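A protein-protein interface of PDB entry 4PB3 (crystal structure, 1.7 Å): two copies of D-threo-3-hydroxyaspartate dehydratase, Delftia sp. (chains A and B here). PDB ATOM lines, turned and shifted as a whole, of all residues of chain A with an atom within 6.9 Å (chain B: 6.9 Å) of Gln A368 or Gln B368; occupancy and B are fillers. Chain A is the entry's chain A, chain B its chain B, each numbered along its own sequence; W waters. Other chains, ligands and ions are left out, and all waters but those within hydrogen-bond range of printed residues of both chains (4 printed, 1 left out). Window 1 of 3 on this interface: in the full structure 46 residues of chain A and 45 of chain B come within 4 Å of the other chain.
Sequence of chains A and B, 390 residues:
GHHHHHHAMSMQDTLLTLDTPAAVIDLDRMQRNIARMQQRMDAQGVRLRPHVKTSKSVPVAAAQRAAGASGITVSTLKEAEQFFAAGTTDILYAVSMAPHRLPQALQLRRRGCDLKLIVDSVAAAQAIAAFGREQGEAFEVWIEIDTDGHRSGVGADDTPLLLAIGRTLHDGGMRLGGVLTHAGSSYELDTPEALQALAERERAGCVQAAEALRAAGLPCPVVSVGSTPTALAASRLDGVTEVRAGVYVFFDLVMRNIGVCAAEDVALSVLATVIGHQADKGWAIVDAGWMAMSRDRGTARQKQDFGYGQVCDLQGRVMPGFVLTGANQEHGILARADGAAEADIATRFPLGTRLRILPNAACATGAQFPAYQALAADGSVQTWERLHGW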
ATOM      1  N   TRP A 290      -1.075  -8.102   6.052  1.00  0.00           N
ATOM      2  CA  TRP A 290      -0.793  -9.494   6.009  1.00  0.00           C
ATOM      3  C   TRP A 290       0.230  -9.822   4.958  1.00  0.00           C
ATOM      4  O   TRP A 290       0.851 -10.885   5.017  1.00  0.00           O
ATOM      5  CB  TRP A 290      -2.088 -10.349   5.844  1.00  0.00           C
ATOM      6  CG  TRP A 290      -2.860 -10.174   4.548  1.00  0.00           C
ATOM      7  CD1 TRP A 290      -4.077  -9.623   4.438  1.00  0.00           C
ATOM      8  CD2 TRP A 290      -2.502 -10.698   3.224  1.00  0.00           C
ATOM      9  NE1 TRP A 290      -4.507  -9.704   3.106  1.00  0.00           N
ATOM     10  CE2 TRP A 290      -3.592 -10.320   2.367  1.00  0.00           C
ATOM     11  CE3 TRP A 290      -1.396 -11.382   2.710  1.00  0.00           C
ATOM     12  CZ2 TRP A 290      -3.603 -10.629   0.986  1.00  0.00           C
ATOM     13  CZ3 TRP A 290      -1.338 -11.686   1.302  1.00  0.00           C
ATOM     14  CH2 TRP A 290      -2.432 -11.322   0.479  1.00  0.00           C
ATOM     15  N   MET A 291       0.503  -8.958   3.928  1.00  0.00           N
ATOM     16  CA  MET A 291       1.638  -9.289   3.018  1.00  0.00           C
ATOM     17  C   MET A 291       2.964  -9.183   3.751  1.00  0.00           C
ATOM     18  O   MET A 291       3.882  -9.948   3.466  1.00  0.00           O
ATOM     19  CB  MET A 291       1.586  -8.319   1.773  1.00  0.00           C
ATOM     20  CG  MET A 291       2.598  -8.724   0.710  1.00  0.00           C
ATOM     21  SD  MET A 291       2.253 -10.394  -0.007  1.00  0.00           S
ATOM     22  CE  MET A 291       0.802  -9.898  -1.016  1.00  0.00           C
ATOM     23  N   ALA A 292       3.028  -8.328   4.800  1.00  0.00           N
ATOM     24  CA  ALA A 292       4.283  -8.342   5.580  1.00  0.00           C
ATOM     25  C   ALA A 292       4.223  -9.452   6.681  1.00  0.00           C
ATOM     26  O   ALA A 292       5.245 -10.146   6.847  1.00  0.00           O
ATOM     27  CB  ALA A 292       4.452  -6.995   6.335  1.00  0.00           C
ATOM     28  N   MET A 293       3.110  -9.567   7.410  1.00  0.00           N
ATOM     29  CA  MET A 293       3.107 -10.504   8.539  1.00  0.00           C
ATOM     30  C   MET A 293       2.905 -11.966   8.085  1.00  0.00           C
ATOM     31  O   MET A 293       3.180 -12.917   8.895  1.00  0.00           O
ATOM     32  CB  MET A 293       1.977 -10.117   9.489  1.00  0.00           C
ATOM     33  CG  MET A 293       2.150  -8.701  10.102  1.00  0.00           C
ATOM     34  SD  MET A 293       3.804  -8.253  10.740  1.00  0.00           S
ATOM     35  CE  MET A 293       4.093  -9.538  11.998  1.00  0.00           C
ATOM     36  N   SER A 294       2.430 -12.138   6.841  1.00  0.00           N
ATOM     37  CA  SER A 294       1.723 -13.392   6.428  1.00  0.00           C
ATOM     38  C   SER A 294       0.329 -13.517   7.065  1.00  0.00           C
ATOM     39  O   SER A 294      -0.053 -12.872   8.054  1.00  0.00           O
ATOM     40  CB  SER A 294       2.593 -14.690   6.703  1.00  0.00           C
ATOM     41  OG  SER A 294       2.280 -15.198   8.013  1.00  0.00           O
ATOM     42  N   ARG A 295      -0.398 -14.509   6.487  1.00  0.00           N
ATOM     43  CA  ARG A 295      -1.752 -14.807   6.984  1.00  0.00           C
ATOM     44  C   ARG A 295      -1.740 -15.777   8.204  1.00  0.00           C
ATOM     45  O   ARG A 295      -2.811 -16.211   8.630  1.00  0.00           O
ATOM     46  CB  ARG A 295      -2.581 -15.435   5.844  1.00  0.00           C
ATOM     47  CG  ARG A 295      -3.249 -14.334   4.938  1.00  0.00           C
ATOM     48  CD  ARG A 295      -4.331 -13.561   5.754  1.00  0.00           C
ATOM     49  NE  ARG A 295      -5.324 -13.008   4.809  1.00  0.00           N
ATOM     50  CZ  ARG A 295      -6.161 -12.018   5.145  1.00  0.00           C
ATOM     51  NH1 ARG A 295      -6.229 -11.517   6.396  1.00  0.00           N
ATOM     52  NH2 ARG A 295      -7.048 -11.558   4.242  1.00  0.00           N
ATOM     53  N   CYS A 363       8.518 -18.646  10.687  1.00  0.00           N
ATOM     54  CA  CYS A 363       8.777 -19.273   9.372  1.00  0.00           C
ATOM     55  C   CYS A 363       7.870 -18.625   8.292  1.00  0.00           C
ATOM     56  O   CYS A 363       8.297 -18.470   7.120  1.00  0.00           O
ATOM     57  CB  CYS A 363       8.327 -20.737   9.378  1.00  0.00           C
ATOM     58  SG  CYS A 363       9.542 -21.782  10.326  1.00  0.00           S
ATOM     59  N   ALA A 364       6.651 -18.245   8.681  1.00  0.00           N
ATOM     60  CA  ALA A 364       5.668 -17.750   7.693  1.00  0.00           C
ATOM     61  C   ALA A 364       5.996 -16.253   7.397  1.00  0.00           C
ATOM     62  O   ALA A 364       6.017 -15.809   6.239  1.00  0.00           O
ATOM     63  CB  ALA A 364       4.209 -17.887   8.265  1.00  0.00           C
ATOM     64  N   THR A 365       6.203 -15.475   8.498  1.00  0.00           N
ATOM     65  CA  THR A 365       6.510 -14.039   8.275  1.00  0.00           C
ATOM     66  C   THR A 365       7.800 -13.876   7.482  1.00  0.00           C
ATOM     67  O   THR A 365       7.846 -13.044   6.553  1.00  0.00           O
ATOM     68  CB  THR A 365       6.595 -13.367   9.649  1.00  0.00           C
ATOM     69  OG1 THR A 365       5.306 -13.399  10.305  1.00  0.00           O
ATOM     70  CG2 THR A 365       7.053 -11.855   9.467  1.00  0.00           C
ATOM     71  N   GLY A 366       8.877 -14.641   7.835  1.00  0.00           N
ATOM     72  CA  GLY A 366      10.174 -14.469   7.151  1.00  0.00           C
ATOM     73  C   GLY A 366      10.019 -14.629   5.600  1.00  0.00           C
ATOM     74  O   GLY A 366      10.668 -13.902   4.867  1.00  0.00           O
ATOM     75  N   ALA A 367       9.191 -15.608   5.218  1.00  0.00           N
ATOM     76  CA  ALA A 367       9.010 -15.928   3.807  1.00  0.00           C
ATOM     77  C   ALA A 367       8.392 -14.788   2.994  1.00  0.00           C
ATOM     78  O   ALA A 367       8.518 -14.801   1.747  1.00  0.00           O
ATOM     79  CB  ALA A 367       8.206 -17.232   3.619  1.00  0.00           C
ATOM     80  N   GLN A 368       7.748 -13.851   3.654  1.00  0.00           N
ATOM     81  CA  GLN A 368       7.194 -12.701   2.953  1.00  0.00           C
ATOM     82  C   GLN A 368       8.243 -11.697   2.506  1.00  0.00           C
ATOM     83  O   GLN A 368       7.905 -10.770   1.755  1.00  0.00           O
ATOM     84  CB  GLN A 368       6.180 -11.999   3.888  1.00  0.00           C
ATOM     85  CG  GLN A 368       5.008 -12.920   4.275  1.00  0.00           C
ATOM     86  CD  GLN A 368       4.292 -13.540   3.064  1.00  0.00           C
ATOM     87  OE1 GLN A 368       4.635 -14.656   2.604  1.00  0.00           O
ATOM     88  NE2 GLN A 368       3.237 -12.885   2.621  1.00  0.00           N
ATOM     89  N   PHE A 369       9.503 -11.824   2.995  1.00  0.00           N
ATOM     90  CA  PHE A 369      10.491 -10.791   2.676  1.00  0.00           C
ATOM     91  C   PHE A 369      11.650 -11.335   1.816  1.00  0.00           C
ATOM     92  O   PHE A 369      12.119 -12.489   2.001  1.00  0.00           O
ATOM     93  CB  PHE A 369      11.141 -10.297   4.012  1.00  0.00           C
ATOM     94  CG  PHE A 369      10.175  -9.485   4.804  1.00  0.00           C
ATOM     95  CD1 PHE A 369       9.300 -10.139   5.635  1.00  0.00           C
ATOM     96  CD2 PHE A 369      10.163  -8.119   4.669  1.00  0.00           C
ATOM     97  CE1 PHE A 369       8.342  -9.381   6.397  1.00  0.00           C
ATOM     98  CE2 PHE A 369       9.172  -7.313   5.393  1.00  0.00           C
ATOM     99  CZ  PHE A 369       8.295  -8.017   6.251  1.00  0.00           C
ATOM    100  N   PRO A 370      12.157 -10.520   0.911  1.00  0.00           N
ATOM    101  CA  PRO A 370      13.316 -10.924   0.116  1.00  0.00           C
ATOM    102  C   PRO A 370      14.571 -11.010   0.975  1.00  0.00           C
ATOM    103  O   PRO A 370      15.519 -11.684   0.561  1.00  0.00           O
ATOM    104  CB  PRO A 370      13.477  -9.738  -0.875  1.00  0.00           C
ATOM    105  CG  PRO A 370      12.069  -9.271  -1.118  1.00  0.00           C
ATOM    106  CD  PRO A 370      11.420  -9.334   0.284  1.00  0.00           C
ATOM    107  N   ALA A 371      14.542 -10.274   2.086  1.00  0.00           N
ATOM    108  CA  ALA A 371      15.796 -10.203   2.916  1.00  0.00           C
ATOM    109  C   ALA A 371      15.420  -9.761   4.294  1.00  0.00           C
ATOM    110  O   ALA A 371      14.347  -9.183   4.535  1.00  0.00           O
ATOM    111  CB  ALA A 371      16.762  -9.168   2.322  1.00  0.00           C
ATOM    112  N   ARG A 386      17.420 -13.721   1.749  1.00  0.00           N
ATOM    113  CA  ARG A 386      16.971 -15.098   2.008  1.00  0.00           C
ATOM    114  C   ARG A 386      16.262 -15.621   0.789  1.00  0.00           C
ATOM    115  O   ARG A 386      15.902 -14.815  -0.125  1.00  0.00           O
ATOM    116  CB  ARG A 386      16.060 -15.179   3.231  1.00  0.00           C
ATOM    117  CG  ARG A 386      14.788 -14.244   3.099  1.00  0.00           C
ATOM    118  CD  ARG A 386      13.699 -14.790   4.043  1.00  0.00           C
ATOM    119  NE  ARG A 386      13.098 -16.035   3.477  1.00  0.00           N
ATOM    120  CZ  ARG A 386      12.496 -16.998   4.203  1.00  0.00           C
ATOM    121  NH1 ARG A 386      11.888 -18.043   3.577  1.00  0.00           N
ATOM    122  NH2 ARG A 386      12.548 -17.027   5.551  1.00  0.00           N
ATOM    123  N   HIS A 388      13.395 -17.392  -1.723  1.00  0.00           N
ATOM    124  CA  HIS A 388      11.958 -17.448  -1.954  1.00  0.00           C
ATOM    125  C   HIS A 388      11.755 -18.485  -3.065  1.00  0.00           C
ATOM    126  O   HIS A 388      12.488 -18.450  -4.076  1.00  0.00           O
ATOM    127  CB  HIS A 388      11.580 -16.033  -2.574  1.00  0.00           C
ATOM    128  CG  HIS A 388      10.118 -15.808  -2.765  1.00  0.00           C
ATOM    129  ND1 HIS A 388       9.637 -15.206  -3.891  1.00  0.00           N
ATOM    130  CD2 HIS A 388       9.048 -16.104  -1.968  1.00  0.00           C
ATOM    131  CE1 HIS A 388       8.296 -15.071  -3.762  1.00  0.00           C
ATOM    132  NE2 HIS A 388       7.931 -15.634  -2.582  1.00  0.00           N
ATOM    133  N   GLY A 389      10.689 -19.288  -2.951  1.00  0.00           N
ATOM    134  CA  GLY A 389      10.269 -20.135  -4.100  1.00  0.00           C
ATOM    135  C   GLY A 389      10.882 -21.510  -4.117  1.00  0.00           C
ATOM    136  O   GLY A 389      11.315 -22.002  -3.038  1.00  0.00           O
ATOM    137  N   TRP A 390      10.920 -22.163  -5.284  1.00  0.00           N
ATOM    138  CA  TRP A 390      11.284 -23.590  -5.399  1.00  0.00           C
ATOM    139  C   TRP A 390      12.223 -23.787  -6.534  1.00  0.00           C
ATOM    140  O   TRP A 390      12.439 -22.847  -7.356  1.00  0.00           O
ATOM    141  CB  TRP A 390      10.008 -24.437  -5.704  1.00  0.00           C
ATOM    142  CG  TRP A 390       9.098 -24.451  -4.478  1.00  0.00           C
ATOM    143  CD1 TRP A 390       9.130 -25.332  -3.433  1.00  0.00           C
ATOM    144  CD2 TRP A 390       8.135 -23.436  -4.118  1.00  0.00           C
ATOM    145  NE1 TRP A 390       8.189 -25.024  -2.500  1.00  0.00           N
ATOM    146  CE2 TRP A 390       7.581 -23.848  -2.822  1.00  0.00           C
ATOM    147  CE3 TRP A 390       7.637 -22.277  -4.757  1.00  0.00           C
ATOM    148  CZ2 TRP A 390       6.586 -23.122  -2.192  1.00  0.00           C
ATOM    149  CZ3 TRP A 390       6.725 -21.495  -4.072  1.00  0.00           C
ATOM    150  CH2 TRP A 390       6.184 -21.912  -2.833  1.00  0.00           C
ATOM    151  OXT TRP A 390      12.801 -24.888  -6.664  1.00  0.00           O
ATOM    152  N   TRP B 290       1.460 -24.870   3.034  1.00  0.00           N
ATOM    153  CA  TRP B 290       1.112 -23.494   3.142  1.00  0.00           C
ATOM    154  C   TRP B 290       2.097 -22.519   2.532  1.00  0.00           C
ATOM    155  O   TRP B 290       1.799 -21.367   2.228  1.00  0.00           O
ATOM    156  CB  TRP B 290       0.663 -23.026   4.583  1.00  0.00           C
ATOM    157  CG  TRP B 290       1.771 -23.130   5.634  1.00  0.00           C
ATOM    158  CD1 TRP B 290       1.840 -24.072   6.615  1.00  0.00           C
ATOM    159  CD2 TRP B 290       2.913 -22.244   5.789  1.00  0.00           C
ATOM    160  NE1 TRP B 290       2.966 -23.832   7.395  1.00  0.00           N
ATOM    161  CE2 TRP B 290       3.674 -22.759   6.943  1.00  0.00           C
ATOM    162  CE3 TRP B 290       3.375 -21.127   5.125  1.00  0.00           C
ATOM    163  CZ2 TRP B 290       4.883 -22.147   7.359  1.00  0.00           C
ATOM    164  CZ3 TRP B 290       4.594 -20.459   5.547  1.00  0.00           C
ATOM    165  CH2 TRP B 290       5.325 -20.994   6.647  1.00  0.00           C
ATOM    166  N   MET B 291       3.368 -23.000   2.345  1.00  0.00           N
ATOM    167  CA  MET B 291       4.280 -22.073   1.741  1.00  0.00           C
ATOM    168  C   MET B 291       3.883 -21.940   0.244  1.00  0.00           C
ATOM    169  O   MET B 291       4.120 -20.860  -0.287  1.00  0.00           O
ATOM    170  CB  MET B 291       5.724 -22.634   1.788  1.00  0.00           C
ATOM    171  CG  MET B 291       6.767 -21.595   1.252  1.00  0.00           C
ATOM    172  SD  MET B 291       6.833 -20.096   2.270  1.00  0.00           S
ATOM    173  CE  MET B 291       7.735 -20.768   3.744  1.00  0.00           C
ATOM    174  N   ALA B 292       3.273 -22.948  -0.343  1.00  0.00           N
ATOM    175  CA  ALA B 292       2.720 -22.755  -1.718  1.00  0.00           C
ATOM    176  C   ALA B 292       1.337 -22.097  -1.718  1.00  0.00           C
ATOM    177  O   ALA B 292       1.113 -21.160  -2.493  1.00  0.00           O
ATOM    178  CB  ALA B 292       2.647 -24.114  -2.429  1.00  0.00           C
ATOM    179  N   MET B 293       0.437 -22.570  -0.843  1.00  0.00           N
ATOM    180  CA  MET B 293      -0.942 -22.047  -0.859  1.00  0.00           C
ATOM    181  C   MET B 293      -1.087 -20.670  -0.150  1.00  0.00           C
ATOM    182  O   MET B 293      -2.047 -19.912  -0.445  1.00  0.00           O
ATOM    183  CB  MET B 293      -1.866 -23.039  -0.146  1.00  0.00           C
ATOM    184  CG  MET B 293      -1.968 -24.417  -0.843  1.00  0.00           C
ATOM    185  SD  MET B 293      -2.045 -24.394  -2.702  1.00  0.00           S
ATOM    186  CE  MET B 293      -3.537 -23.402  -3.021  1.00  0.00           C
ATOM    187  N   SER B 294      -0.112 -20.369   0.705  1.00  0.00           N
ATOM    188  CA  SER B 294      -0.285 -19.300   1.698  1.00  0.00           C
ATOM    189  C   SER B 294      -1.143 -19.817   2.853  1.00  0.00           C
ATOM    190  O   SER B 294      -1.866 -20.803   2.739  1.00  0.00           O
ATOM    191  CB  SER B 294      -0.867 -17.955   1.097  1.00  0.00           C
ATOM    192  OG  SER B 294      -2.268 -17.887   1.327  1.00  0.00           O
ATOM    193  N   ARG B 295      -1.034 -19.039   3.971  1.00  0.00           N
ATOM    194  CA  ARG B 295      -1.864 -19.376   5.148  1.00  0.00           C
ATOM    195  C   ARG B 295      -3.317 -18.812   5.051  1.00  0.00           C
ATOM    196  O   ARG B 295      -4.079 -19.050   6.007  1.00  0.00           O
ATOM    197  CB  ARG B 295      -1.234 -18.834   6.460  1.00  0.00           C
ATOM    198  CG  ARG B 295      -0.123 -19.807   6.994  1.00  0.00           C
ATOM    199  CD  ARG B 295      -0.793 -21.060   7.518  1.00  0.00           C
ATOM    200  NE  ARG B 295       0.102 -21.646   8.554  1.00  0.00           N
ATOM    201  CZ  ARG B 295      -0.013 -22.891   8.999  1.00  0.00           C
ATOM    202  NH1 ARG B 295      -1.001 -23.685   8.548  1.00  0.00           N
ATOM    203  NH2 ARG B 295       0.837 -23.438   9.930  1.00  0.00           N
ATOM    204  N   CYS B 363      -4.656 -13.362  -4.284  1.00  0.00           N
ATOM    205  CA  CYS B 363      -3.675 -12.333  -3.998  1.00  0.00           C
ATOM    206  C   CYS B 363      -2.646 -12.964  -3.040  1.00  0.00           C
ATOM    207  O   CYS B 363      -1.452 -12.595  -3.100  1.00  0.00           O
ATOM    208  CB  CYS B 363      -4.292 -11.213  -3.197  1.00  0.00           C
ATOM    209  SG  CYS B 363      -5.239 -10.008  -4.217  1.00  0.00           S
ATOM    210  N   ALA B 364      -3.108 -13.803  -2.097  1.00  0.00           N
ATOM    211  CA  ALA B 364      -2.190 -14.376  -1.101  1.00  0.00           C
ATOM    212  C   ALA B 364      -1.347 -15.578  -1.645  1.00  0.00           C
ATOM    213  O   ALA B 364      -0.085 -15.582  -1.520  1.00  0.00           O
ATOM    214  CB  ALA B 364      -3.000 -14.830   0.129  1.00  0.00           C
ATOM    215  N   THR B 365      -2.057 -16.468  -2.362  1.00  0.00           N
ATOM    216  CA  THR B 365      -1.296 -17.542  -3.070  1.00  0.00           C
ATOM    217  C   THR B 365      -0.284 -17.012  -4.022  1.00  0.00           C
ATOM    218  O   THR B 365       0.859 -17.495  -4.059  1.00  0.00           O
ATOM    219  CB  THR B 365      -2.288 -18.478  -3.722  1.00  0.00           C
ATOM    220  OG1 THR B 365      -3.154 -19.045  -2.687  1.00  0.00           O
ATOM    221  CG2 THR B 365      -1.554 -19.627  -4.463  1.00  0.00           C
ATOM    222  N   GLY B 366      -0.676 -16.083  -4.900  1.00  0.00           N
ATOM    223  CA  GLY B 366       0.332 -15.586  -5.907  1.00  0.00           C
ATOM    224  C   GLY B 366       1.615 -15.072  -5.273  1.00  0.00           C
ATOM    225  O   GLY B 366       2.671 -15.275  -5.863  1.00  0.00           O
ATOM    226  N   ALA B 367       1.533 -14.359  -4.143  1.00  0.00           N
ATOM    227  CA  ALA B 367       2.741 -13.742  -3.567  1.00  0.00           C
ATOM    228  C   ALA B 367       3.725 -14.781  -3.073  1.00  0.00           C
ATOM    229  O   ALA B 367       4.861 -14.406  -2.764  1.00  0.00           O
ATOM    230  CB  ALA B 367       2.267 -12.824  -2.399  1.00  0.00           C
ATOM    231  N   GLN B 368       3.283 -16.036  -2.951  1.00  0.00           N
ATOM    232  CA  GLN B 368       4.246 -17.096  -2.501  1.00  0.00           C
ATOM    233  C   GLN B 368       5.199 -17.532  -3.607  1.00  0.00           C
ATOM    234  O   GLN B 368       6.172 -18.259  -3.341  1.00  0.00           O
ATOM    235  CB  GLN B 368       3.479 -18.311  -2.004  1.00  0.00           C
ATOM    236  CG  GLN B 368       2.625 -17.951  -0.804  1.00  0.00           C
ATOM    237  CD  GLN B 368       3.452 -17.350   0.308  1.00  0.00           C
ATOM    238  OE1 GLN B 368       3.486 -16.127   0.477  1.00  0.00           O
ATOM    239  NE2 GLN B 368       4.065 -18.224   1.145  1.00  0.00           N
ATOM    240  N   PHE B 369       4.970 -17.047  -4.843  1.00  0.00           N
ATOM    241  CA  PHE B 369       5.784 -17.559  -5.966  1.00  0.00           C
ATOM    242  C   PHE B 369       6.589 -16.442  -6.652  1.00  0.00           C
ATOM    243  O   PHE B 369       6.065 -15.319  -6.886  1.00  0.00           O
ATOM    244  CB  PHE B 369       4.844 -18.141  -7.048  1.00  0.00           C
ATOM    245  CG  PHE B 369       4.188 -19.419  -6.584  1.00  0.00           C
ATOM    246  CD1 PHE B 369       2.989 -19.349  -5.815  1.00  0.00           C
ATOM    247  CD2 PHE B 369       4.766 -20.660  -6.923  1.00  0.00           C
ATOM    248  CE1 PHE B 369       2.379 -20.532  -5.397  1.00  0.00           C
ATOM    249  CE2 PHE B 369       4.197 -21.862  -6.460  1.00  0.00           C
ATOM    250  CZ  PHE B 369       3.021 -21.736  -5.667  1.00  0.00           C
ATOM    251  N   PRO B 370       7.860 -16.754  -7.029  1.00  0.00           N
ATOM    252  CA  PRO B 370       8.646 -15.767  -7.823  1.00  0.00           C
ATOM    253  C   PRO B 370       8.015 -15.493  -9.195  1.00  0.00           C
ATOM    254  O   PRO B 370       8.237 -14.366  -9.727  1.00  0.00           O
ATOM    255  CB  PRO B 370      10.001 -16.457  -8.029  1.00  0.00           C
ATOM    256  CG  PRO B 370      10.117 -17.367  -6.753  1.00  0.00           C
ATOM    257  CD  PRO B 370       8.722 -17.896  -6.548  1.00  0.00           C
ATOM    258  N   ALA B 371       7.266 -16.459  -9.690  1.00  0.00           N
ATOM    259  CA  ALA B 371       6.750 -16.393 -11.085  1.00  0.00           C
ATOM    260  C   ALA B 371       5.550 -17.256 -11.203  1.00  0.00           C
ATOM    261  O   ALA B 371       5.406 -18.245 -10.484  1.00  0.00           O
ATOM    262  CB  ALA B 371       7.807 -16.855 -12.041  1.00  0.00           C
ATOM    263  N   ARG B 386       6.837 -12.250 -11.280  1.00  0.00           N
ATOM    264  CA  ARG B 386       6.027 -11.253 -10.546  1.00  0.00           C
ATOM    265  C   ARG B 386       6.891 -10.686  -9.401  1.00  0.00           C
ATOM    266  O   ARG B 386       7.915 -11.289  -9.050  1.00  0.00           O
ATOM    267  CB  ARG B 386       4.747 -11.859  -9.997  1.00  0.00           C
ATOM    268  CG  ARG B 386       4.946 -13.047  -9.019  1.00  0.00           C
ATOM    269  CD  ARG B 386       3.636 -13.138  -8.153  1.00  0.00           C
ATOM    270  NE  ARG B 386       3.602 -12.118  -7.147  1.00  0.00           N
ATOM    271  CZ  ARG B 386       2.494 -11.675  -6.534  1.00  0.00           C
ATOM    272  NH1 ARG B 386       2.598 -10.835  -5.486  1.00  0.00           N
ATOM    273  NH2 ARG B 386       1.243 -11.997  -6.963  1.00  0.00           N
ATOM    274  N   HIS B 388       8.108  -9.551  -5.671  1.00  0.00           N
ATOM    275  CA  HIS B 388       8.010  -9.889  -4.230  1.00  0.00           C
ATOM    276  C   HIS B 388       8.666  -8.807  -3.396  1.00  0.00           C
ATOM    277  O   HIS B 388       9.672  -8.252  -3.762  1.00  0.00           O
ATOM    278  CB  HIS B 388       8.893 -11.168  -4.088  1.00  0.00           C
ATOM    279  CG  HIS B 388       8.843 -11.750  -2.700  1.00  0.00           C
ATOM    280  ND1 HIS B 388       9.993 -12.168  -2.053  1.00  0.00           N
ATOM    281  CD2 HIS B 388       7.758 -12.106  -1.923  1.00  0.00           C
ATOM    282  CE1 HIS B 388       9.603 -12.771  -0.897  1.00  0.00           C
ATOM    283  NE2 HIS B 388       8.269 -12.742  -0.811  1.00  0.00           N
ATOM    284  N   GLY B 389       8.000  -8.466  -2.285  1.00  0.00           N
ATOM    285  CA  GLY B 389       8.663  -7.538  -1.364  1.00  0.00           C
ATOM    286  C   GLY B 389       8.254  -6.068  -1.608  1.00  0.00           C
ATOM    287  O   GLY B 389       7.156  -5.780  -2.209  1.00  0.00           O
ATOM    288  N   TRP B 390       9.138  -5.193  -1.206  1.00  0.00           N
ATOM    289  CA  TRP B 390       8.883  -3.730  -1.161  1.00  0.00           C
ATOM    290  C   TRP B 390      10.025  -2.979  -1.690  1.00  0.00           C
ATOM    291  O   TRP B 390      11.089  -3.528  -2.078  1.00  0.00           O
ATOM    292  CB  TRP B 390       8.615  -3.251   0.318  1.00  0.00           C
ATOM    293  CG  TRP B 390       7.366  -3.873   0.883  1.00  0.00           C
ATOM    294  CD1 TRP B 390       6.094  -3.344   0.836  1.00  0.00           C
ATOM    295  CD2 TRP B 390       7.222  -5.193   1.474  1.00  0.00           C
ATOM    296  NE1 TRP B 390       5.175  -4.240   1.383  1.00  0.00           N
ATOM    297  CE2 TRP B 390       5.793  -5.389   1.735  1.00  0.00           C
ATOM    298  CE3 TRP B 390       8.128  -6.247   1.784  1.00  0.00           C
ATOM    299  CZ2 TRP B 390       5.279  -6.547   2.341  1.00  0.00           C
ATOM    300  CZ3 TRP B 390       7.573  -7.436   2.295  1.00  0.00           C
ATOM    301  CH2 TRP B 390       6.176  -7.603   2.585  1.00  0.00           C
ATOM    302  OXT TRP B 390       9.948  -1.743  -1.812  1.00  0.00           O
HETATM  303  O   HOH W   1       1.283 -14.524   0.692  1.00  0.00           O
HETATM  304  O   HOH W   2       6.624 -16.228   0.173  1.00  0.00           O
HETATM  305  O   HOH W   3       4.616 -16.892   4.082  1.00  0.00           O
HETATM  306  O   HOH W   4       5.495  -8.992  -1.269  1.00  0.00           O
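NE2 of His B388 is in hydrogen-bond range of O of Ala A367 (3.3 Å).
The side-chain amide oxygen (OE1) of Gln B368 lies close to the side-chain amide oxygen (OE1) of Gln A368.
The backbone carbonyl oxygen (O) of Gln A368 sits at hydrogen-bond distance from a ring nitrogen (NE2) of His B388 (3.3 Å).
The backbone carbonyl oxygen (O) of Ala B367 lies within hydrogen-bond range of a ring nitrogen (NE2) of His A388, at 3.3 Å.
A ring nitrogen (NE2) of His A388 sits at hydrogen-bond distance from the backbone carbonyl oxygen (O) of Gln B368, 3.2 Å away.
NE2 of His B388 is in hydrogen-bond range of NE2 of His A388 (3.4 Å).
The backbone carbonyl oxygen of Pro A370 sits at hydrogen-bond distance from the backbone NH of Arg A386 (3.0 Å).
O of Met B291 sits at hydrogen-bond distance from NE2 of Gln B368, at 3.0 Å.
O of Pro B370 is in hydrogen-bond range of N of Arg B386, at 3.0 Å.
SD of Met A291 touches CB of Ala B367, at 3.4 Å.
Cys A363 touches Trp B290 (C to CH2, 3.8 Å).
Gly B389 touches Pro A370 (CA to CD, 3.7 Å).
Phe B369 touches His A388.
His A388 touches Pro B370 (ND1 to CG, 3.6 Å).
Gly A389 touches Pro B370.
CZ3 of Trp A390 touches CE2 of Phe B369, 3.5 Å away.
Of the printed residues of chain B, Arg A295 touches Arg B295.
Of the printed residues of chain B, Ala A364 touches Trp B290.
Of the printed residues of chain B, Phe A369 touches His B388 and Trp B390.
Of the printed residues of chain A, Gln B368 touches Gln A368, His A388 and Trp A390.
The nearest printed residue of chain B that does not touch Gln A368 is Gly B389 (4.6 Å).
Printed residues of chain A that touch a printed residue of chain B: Trp A290, Met A291, Ala A292, Arg A295, Cys A363, Ala A364, Ala A367, Gln A368, Phe A369, Pro A370, His A388, Gly A389 and Trp A390.
Of the 19 printed residues of chain B, 13 touch a printed residue of chain A.
Hydrophobic or aromatic side chains of chain B within 4 Å of the printed part of chain A: Trp B290, Met B291, Ala B364, Ala B367, Phe B369, Pro B370, His B388 and Trp B390.
Among the printed residues, no Asp or Glu carboxylate lies within 4 Å of a Lys or Arg side-chain nitrogen of the other chain.
Gln B368 touches its own counterpart, Gln A368.
Phe A369 touches Trp B390, and with the chains exchanged Trp A390 touches Phe B369.
His B388 touches its own counterpart, His A388.
19 positions are printed for both chains.
Water W4 lies within hydrogen-bond range of the backbone NH of Gly B389 (2.8 Å) and the side-chain sulfur of Met A291 (3.8 Å).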
